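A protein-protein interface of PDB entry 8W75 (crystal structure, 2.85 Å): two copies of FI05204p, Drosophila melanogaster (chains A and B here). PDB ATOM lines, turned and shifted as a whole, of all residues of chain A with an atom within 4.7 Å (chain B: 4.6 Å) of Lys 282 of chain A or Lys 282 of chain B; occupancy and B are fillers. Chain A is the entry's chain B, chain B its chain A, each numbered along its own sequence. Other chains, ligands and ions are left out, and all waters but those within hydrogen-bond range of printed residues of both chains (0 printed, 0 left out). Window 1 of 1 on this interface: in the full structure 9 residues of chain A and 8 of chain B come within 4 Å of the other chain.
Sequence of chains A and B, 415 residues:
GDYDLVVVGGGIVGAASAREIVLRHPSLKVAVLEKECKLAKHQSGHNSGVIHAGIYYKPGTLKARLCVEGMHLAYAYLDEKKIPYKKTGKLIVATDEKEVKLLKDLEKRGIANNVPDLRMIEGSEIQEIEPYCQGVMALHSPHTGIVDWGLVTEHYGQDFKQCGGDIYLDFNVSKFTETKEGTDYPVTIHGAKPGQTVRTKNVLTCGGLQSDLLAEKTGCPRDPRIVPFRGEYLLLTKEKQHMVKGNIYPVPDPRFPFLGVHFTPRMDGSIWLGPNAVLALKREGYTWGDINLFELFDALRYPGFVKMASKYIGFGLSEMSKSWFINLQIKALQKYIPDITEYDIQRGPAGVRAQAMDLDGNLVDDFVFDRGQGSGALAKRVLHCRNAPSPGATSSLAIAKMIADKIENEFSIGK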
ATOM      1  N   PRO A 228     -20.115  -7.031  25.615  1.00  0.00           N
ATOM      2  CA  PRO A 228     -18.791  -6.559  26.047  1.00  0.00           C
ATOM      3  C   PRO A 228     -18.713  -6.431  27.564  1.00  0.00           C
ATOM      4  O   PRO A 228     -19.591  -5.840  28.198  1.00  0.00           O
ATOM      5  CB  PRO A 228     -18.663  -5.193  25.364  1.00  0.00           C
ATOM      6  CG  PRO A 228     -20.074  -4.721  25.232  1.00  0.00           C
ATOM      7  CD  PRO A 228     -20.919  -5.953  25.011  1.00  0.00           C
ATOM      8  N   ALA A 280     -19.329  -3.280  29.796  1.00  0.00           N
ATOM      9  CA  ALA A 280     -18.928  -2.164  28.953  1.00  0.00           C
ATOM     10  C   ALA A 280     -20.135  -1.615  28.204  1.00  0.00           C
ATOM     11  O   ALA A 280     -20.882  -2.369  27.573  1.00  0.00           O
ATOM     12  CB  ALA A 280     -17.845  -2.600  27.968  1.00  0.00           C
ATOM     13  N   LEU A 281     -20.326  -0.297  28.277  1.00  0.00           N
ATOM     14  CA  LEU A 281     -21.398   0.377  27.558  1.00  0.00           C
ATOM     15  C   LEU A 281     -21.053   0.630  26.095  1.00  0.00           C
ATOM     16  O   LEU A 281     -21.638   1.523  25.469  1.00  0.00           O
ATOM     17  CB  LEU A 281     -21.749   1.694  28.256  1.00  0.00           C
ATOM     18  CG  LEU A 281     -22.053   1.579  29.752  1.00  0.00           C
ATOM     19  CD1 LEU A 281     -22.515   2.910  30.321  1.00  0.00           C
ATOM     20  CD2 LEU A 281     -23.085   0.491  30.017  1.00  0.00           C
ATOM     21  N   LYS A 282     -20.120  -0.143  25.547  1.00  0.00           N
ATOM     22  CA  LYS A 282     -19.639  -0.009  24.182  1.00  0.00           C
ATOM     23  C   LYS A 282     -18.884  -1.282  23.830  1.00  0.00           C
ATOM     24  O   LYS A 282     -18.246  -1.889  24.696  1.00  0.00           O
ATOM     25  CB  LYS A 282     -18.734   1.221  24.028  1.00  0.00           C
ATOM     26  CG  LYS A 282     -18.289   1.521  22.608  1.00  0.00           C
ATOM     27  CD  LYS A 282     -17.424   2.772  22.562  1.00  0.00           C
ATOM     28  CE  LYS A 282     -17.007   3.108  21.140  1.00  0.00           C
ATOM     29  NZ  LYS A 282     -16.167   4.337  21.083  1.00  0.00           N
ATOM     30  N   ARG A 283     -18.976  -1.686  22.561  1.00  0.00           N
ATOM     31  CA  ARG A 283     -18.295  -2.902  22.119  1.00  0.00           C
ATOM     32  C   ARG A 283     -16.798  -2.822  22.391  1.00  0.00           C
ATOM     33  O   ARG A 283     -16.195  -3.773  22.901  1.00  0.00           O
ATOM     34  CB  ARG A 283     -18.563  -3.143  20.634  1.00  0.00           C
ATOM     35  CG  ARG A 283     -19.940  -3.707  20.339  1.00  0.00           C
ATOM     36  CD  ARG A 283     -20.130  -5.054  21.016  1.00  0.00           C
ATOM     37  NE  ARG A 283     -20.497  -6.092  20.058  1.00  0.00           N
ATOM     38  CZ  ARG A 283     -21.746  -6.386  19.719  1.00  0.00           C
ATOM     39  NH1 ARG A 283     -22.756  -5.720  20.261  1.00  0.00           N
ATOM     40  NH2 ARG A 283     -21.986  -7.346  18.839  1.00  0.00           N
ATOM     41  N   GLU A 284     -16.181  -1.691  22.057  1.00  0.00           N
ATOM     42  CA  GLU A 284     -14.780  -1.468  22.379  1.00  0.00           C
ATOM     43  C   GLU A 284     -14.666  -0.404  23.462  1.00  0.00           C
ATOM     44  O   GLU A 284     -13.867   0.530  23.347  1.00  0.00           O
ATOM     45  CB  GLU A 284     -13.997  -1.062  21.129  1.00  0.00           C
ATOM     46  CG  GLU A 284     -14.118  -2.051  19.982  1.00  0.00           C
ATOM     47  CD  GLU A 284     -13.308  -1.645  18.767  1.00  0.00           C
ATOM     48  OE1 GLU A 284     -13.046  -2.512  17.908  1.00  0.00           O
ATOM     49  OE2 GLU A 284     -12.927  -0.458  18.673  1.00  0.00           O
ATOM     50  N   GLY A 285     -15.470  -0.539  24.515  1.00  0.00           N
ATOM     51  CA  GLY A 285     -15.473   0.426  25.596  1.00  0.00           C
ATOM     52  C   GLY A 285     -14.369   0.201  26.606  1.00  0.00           C
ATOM     53  O   GLY A 285     -14.610  -0.330  27.694  1.00  0.00           O
ATOM     54  N   ASP A 290     -16.703   6.328  27.475  1.00  0.00           N
ATOM     55  CA  ASP A 290     -17.038   6.062  26.082  1.00  0.00           C
ATOM     56  C   ASP A 290     -18.286   5.190  26.007  1.00  0.00           C
ATOM     57  O   ASP A 290     -18.281   4.044  26.464  1.00  0.00           O
ATOM     58  CB  ASP A 290     -15.863   5.390  25.376  1.00  0.00           C
ATOM     59  CG  ASP A 290     -15.796   5.736  23.901  1.00  0.00           C
ATOM     60  OD1 ASP A 290     -16.863   5.974  23.295  1.00  0.00           O
ATOM     61  OD2 ASP A 290     -14.677   5.775  23.348  1.00  0.00           O
ATOM     62  N   ILE A 291     -19.354   5.737  25.427  1.00  0.00           N
ATOM     63  CA  ILE A 291     -20.650   5.075  25.351  1.00  0.00           C
ATOM     64  C   ILE A 291     -21.178   5.197  23.929  1.00  0.00           C
ATOM     65  O   ILE A 291     -21.037   6.245  23.291  1.00  0.00           O
ATOM     66  CB  ILE A 291     -21.652   5.687  26.356  1.00  0.00           C
ATOM     67  CG1 ILE A 291     -21.165   5.494  27.791  1.00  0.00           C
ATOM     68  CG2 ILE A 291     -23.043   5.086  26.179  1.00  0.00           C
ATOM     69  CD1 ILE A 291     -22.036   6.176  28.822  1.00  0.00           C
ATOM     70  N   ASN A 292     -21.782   4.119  23.431  1.00  0.00           N
ATOM     71  CA  ASN A 292     -22.459   4.116  22.139  1.00  0.00           C
ATOM     72  C   ASN A 292     -23.926   3.786  22.368  1.00  0.00           C
ATOM     73  O   ASN A 292     -24.249   2.702  22.867  1.00  0.00           O
ATOM     74  CB  ASN A 292     -21.821   3.109  21.180  1.00  0.00           C
ATOM     75  CG  ASN A 292     -22.412   3.183  19.785  1.00  0.00           C
ATOM     76  OD1 ASN A 292     -23.478   2.627  19.521  1.00  0.00           O
ATOM     77  ND2 ASN A 292     -21.720   3.869  18.884  1.00  0.00           N
ATOM     78  N   GLU A 295     -25.088   0.752  20.272  1.00  0.00           N
ATOM     79  CA  GLU A 295     -24.518  -0.541  20.633  1.00  0.00           C
ATOM     80  C   GLU A 295     -25.135  -1.124  21.895  1.00  0.00           C
ATOM     81  O   GLU A 295     -24.956  -2.317  22.160  1.00  0.00           O
ATOM     82  CB  GLU A 295     -23.002  -0.431  20.797  1.00  0.00           C
ATOM     83  CG  GLU A 295     -22.240  -0.341  19.481  1.00  0.00           C
ATOM     84  CD  GLU A 295     -20.736  -0.371  19.674  1.00  0.00           C
ATOM     85  OE1 GLU A 295     -20.004  -0.437  18.661  1.00  0.00           O
ATOM     86  OE2 GLU A 295     -20.285  -0.330  20.837  1.00  0.00           O
ATOM     87  N   PRO B 228     -16.252  20.040  19.519  1.00  0.00           N
ATOM     88  CA  PRO B 228     -16.507  19.266  18.298  1.00  0.00           C
ATOM     89  C   PRO B 228     -17.870  19.592  17.703  1.00  0.00           C
ATOM     90  O   PRO B 228     -18.889  19.583  18.400  1.00  0.00           O
ATOM     91  CB  PRO B 228     -16.442  17.812  18.780  1.00  0.00           C
ATOM     92  CG  PRO B 228     -16.856  17.888  20.212  1.00  0.00           C
ATOM     93  CD  PRO B 228     -16.346  19.208  20.733  1.00  0.00           C
ATOM     94  N   ALA B 280     -21.106  17.577  18.386  1.00  0.00           N
ATOM     95  CA  ALA B 280     -20.751  16.188  18.627  1.00  0.00           C
ATOM     96  C   ALA B 280     -20.576  15.926  20.116  1.00  0.00           C
ATOM     97  O   ALA B 280     -19.940  16.707  20.828  1.00  0.00           O
ATOM     98  CB  ALA B 280     -19.465  15.834  17.881  1.00  0.00           C
ATOM     99  N   LEU B 281     -21.146  14.813  20.583  1.00  0.00           N
ATOM    100  CA  LEU B 281     -21.019  14.376  21.970  1.00  0.00           C
ATOM    101  C   LEU B 281     -19.695  13.665  22.247  1.00  0.00           C
ATOM    102  O   LEU B 281     -19.612  12.866  23.188  1.00  0.00           O
ATOM    103  CB  LEU B 281     -22.198  13.477  22.346  1.00  0.00           C
ATOM    104  CG  LEU B 281     -23.571  14.099  22.085  1.00  0.00           C
ATOM    105  CD1 LEU B 281     -24.684  13.174  22.535  1.00  0.00           C
ATOM    106  CD2 LEU B 281     -23.687  15.461  22.762  1.00  0.00           C
ATOM    107  N   LYS B 282     -18.662  13.939  21.450  1.00  0.00           N
ATOM    108  CA  LYS B 282     -17.346  13.316  21.555  1.00  0.00           C
ATOM    109  C   LYS B 282     -16.395  14.080  20.645  1.00  0.00           C
ATOM    110  O   LYS B 282     -16.814  14.604  19.609  1.00  0.00           O
ATOM    111  CB  LYS B 282     -17.399  11.832  21.161  1.00  0.00           C
ATOM    112  CG  LYS B 282     -16.121  11.048  21.443  1.00  0.00           C
ATOM    113  CD  LYS B 282     -16.299   9.583  21.088  1.00  0.00           C
ATOM    114  CE  LYS B 282     -15.071   8.782  21.469  1.00  0.00           C
ATOM    115  NZ  LYS B 282     -15.231   7.341  21.139  1.00  0.00           N
ATOM    116  N   ARG B 283     -15.118  14.140  21.036  1.00  0.00           N
ATOM    117  CA  ARG B 283     -14.126  14.827  20.211  1.00  0.00           C
ATOM    118  C   ARG B 283     -14.081  14.240  18.805  1.00  0.00           C
ATOM    119  O   ARG B 283     -14.146  14.972  17.809  1.00  0.00           O
ATOM    120  CB  ARG B 283     -12.745  14.755  20.868  1.00  0.00           C
ATOM    121  CG  ARG B 283     -12.589  15.656  22.079  1.00  0.00           C
ATOM    122  CD  ARG B 283     -12.737  17.116  21.689  1.00  0.00           C
ATOM    123  NE  ARG B 283     -12.579  18.011  22.831  1.00  0.00           N
ATOM    124  CZ  ARG B 283     -11.426  18.570  23.189  1.00  0.00           C
ATOM    125  NH1 ARG B 283     -10.325  18.326  22.492  1.00  0.00           N
ATOM    126  NH2 ARG B 283     -11.376  19.373  24.242  1.00  0.00           N
ATOM    127  N   GLU B 284     -13.977  12.917  18.704  1.00  0.00           N
ATOM    128  CA  GLU B 284     -14.041  12.210  17.427  1.00  0.00           C
ATOM    129  C   GLU B 284     -15.393  11.540  17.228  1.00  0.00           C
ATOM    130  O   GLU B 284     -15.474  10.402  16.759  1.00  0.00           O
ATOM    131  CB  GLU B 284     -12.914  11.188  17.329  1.00  0.00           C
ATOM    132  CG  GLU B 284     -11.522  11.796  17.338  1.00  0.00           C
ATOM    133  CD  GLU B 284     -10.431  10.755  17.183  1.00  0.00           C
ATOM    134  OE1 GLU B 284     -10.758   9.550  17.147  1.00  0.00           O
ATOM    135  OE2 GLU B 284      -9.247  11.142  17.093  1.00  0.00           O
ATOM    136  N   GLY B 285     -16.473  12.232  17.583  1.00  0.00           N
ATOM    137  CA  GLY B 285     -17.805  11.676  17.446  1.00  0.00           C
ATOM    138  C   GLY B 285     -18.371  11.819  16.050  1.00  0.00           C
ATOM    139  O   GLY B 285     -19.120  12.760  15.769  1.00  0.00           O
ATOM    140  N   ASP B 290     -22.294   7.951  19.419  1.00  0.00           N
ATOM    141  CA  ASP B 290     -21.004   7.800  20.088  1.00  0.00           C
ATOM    142  C   ASP B 290     -20.825   8.927  21.099  1.00  0.00           C
ATOM    143  O   ASP B 290     -20.686  10.094  20.723  1.00  0.00           O
ATOM    144  CB  ASP B 290     -19.876   7.794  19.061  1.00  0.00           C
ATOM    145  CG  ASP B 290     -18.645   7.056  19.554  1.00  0.00           C
ATOM    146  OD1 ASP B 290     -18.683   6.521  20.683  1.00  0.00           O
ATOM    147  OD2 ASP B 290     -17.643   7.007  18.811  1.00  0.00           O
ATOM    148  N   ASN B 292     -18.838  10.267  24.739  1.00  0.00           N
ATOM    149  CA  ASN B 292     -17.748  10.159  25.703  1.00  0.00           C
ATOM    150  C   ASN B 292     -18.078  11.075  26.873  1.00  0.00           C
ATOM    151  O   ASN B 292     -17.974  12.300  26.754  1.00  0.00           O
ATOM    152  CB  ASN B 292     -16.407  10.530  25.071  1.00  0.00           C
ATOM    153  CG  ASN B 292     -15.232  10.196  25.966  1.00  0.00           C
ATOM    154  OD1 ASN B 292     -14.920  10.931  26.902  1.00  0.00           O
ATOM    155  ND2 ASN B 292     -14.566   9.083  25.678  1.00  0.00           N
ATOM    156  N   GLU B 295     -15.260  13.580  27.724  1.00  0.00           N
ATOM    157  CA  GLU B 295     -15.137  14.632  26.723  1.00  0.00           C
ATOM    158  C   GLU B 295     -16.421  15.433  26.538  1.00  0.00           C
ATOM    159  O   GLU B 295     -16.364  16.523  25.956  1.00  0.00           O
ATOM    160  CB  GLU B 295     -14.707  14.032  25.383  1.00  0.00           C
ATOM    161  CG  GLU B 295     -13.354  13.348  25.425  1.00  0.00           C
ATOM    162  CD  GLU B 295     -12.940  12.804  24.076  1.00  0.00           C
ATOM    163  OE1 GLU B 295     -11.734  12.550  23.883  1.00  0.00           O
ATOM    164  OE2 GLU B 295     -13.822  12.634  23.208  1.00  0.00           O
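Among the printed residues, Asp or Glu carboxylates within 4 Å of a Lys or Arg side-chain nitrogen of the other chain: Lys 282 of chain A with Asp 290 of chain B (3.4 Å) and Asp 290 of chain A with Lys 282 of chain B (2.8 Å).
The backbone NH (N) of Asn 292 of chain B is in hydrogen-bond range of the backbone carbonyl oxygen (O) of Leu 281 of chain B (3.1 Å).
The side-chain amino group of Lys 282 of chain B lies within salt-bridge range of the side-chain carboxylate of Asp 290 of chain B (3.4 Å).
OD1 of Asn 292 of chain B is in hydrogen-bond range of N of Glu 295 of chain B (2.8 Å).
The side-chain carboxylate (OD1) of Asp 290 of chain A lies within salt-bridge range of the side-chain amino group (NZ) of Lys 282 of chain A, 2.8 Å away.
Lys 282 of chain A touches just these residues of chain B: Lys 282 and Asp 290.
Lys 282 of chain B touches just these residues of chain A: Lys 282 and Asp 290.
Of the printed residues of chain A, Asn 292 of chain B touches Asp 290 (3.9 Å).
Printed residues of chain B within 4 Å of Asp 290 of chain A: Lys 282 (2.8 Å), Asp 290 (3.2 Å) and Asn 292 (3.9 Å).
Of the printed residues of chain B, Ile 291 of chain A touches Asp 290 (3.5 Å).
Of the printed residues of chain A, Asp 290 of chain B touches Lys 282 (3.4 Å), Asp 290 (3.2 Å) and Ile 291 (3.5 Å).
Pro 228 of chain B touches none of the printed residues of chain A.
The nearest printed residue of chain B that does not touch Lys 282 of chain A is Asn 292 of chain B (6.8 Å).
The nearest printed residue of chain A that does not touch Asp 290 of chain B is Asn 292 of chain A (4.2 Å).
The side-chain amino group (NZ) of Lys 282 of chain B lies within salt-bridge range of the side-chain carboxylate (OD2) of Asp 290 of chain A (2.8 Å).
OD1 of Asp 290 of chain B is in salt-bridge range of NZ of Lys 282 of chain A, at 3.4 Å.
NZ of Lys 282 of chain A lies close to NZ of Lys 282 of chain B, at 3.1 Å.
OD1 of Asp 290 of chain B lies close to OD1 of Asp 290 of chain A, at 3.2 Å.
Among the printed residues, pairs that only touch across the chains: Asp 290 of chain A with Asn 292 of chain B (3.9 Å) and Ile 291 of chain A with Asp 290 of chain B (3.5 Å).
Lys 282 of chain A touches its own counterpart, Lys 282 of chain B.
Lys 282 of chain A touches Asp 290 of chain B, and with the chains exchanged Asp 290 of chain A touches Lys 282 of chain B.
Asp 290 of chain B touches its own counterpart, Asp 290 of chain A.
Asp 290 of chain A touches Asn 292 of chain B, but with the chains exchanged Asn 292 of chain A does not touch Asp 290 of chain B (4.2 Å).
Positions printed for both chains: 228, 280, 281, 282, 283, 284, 285, 290, 292 and 295.
Of the 6 pairs that touch across the chains among the printed residues, 4 have their exchanged pair printed and touching as well.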
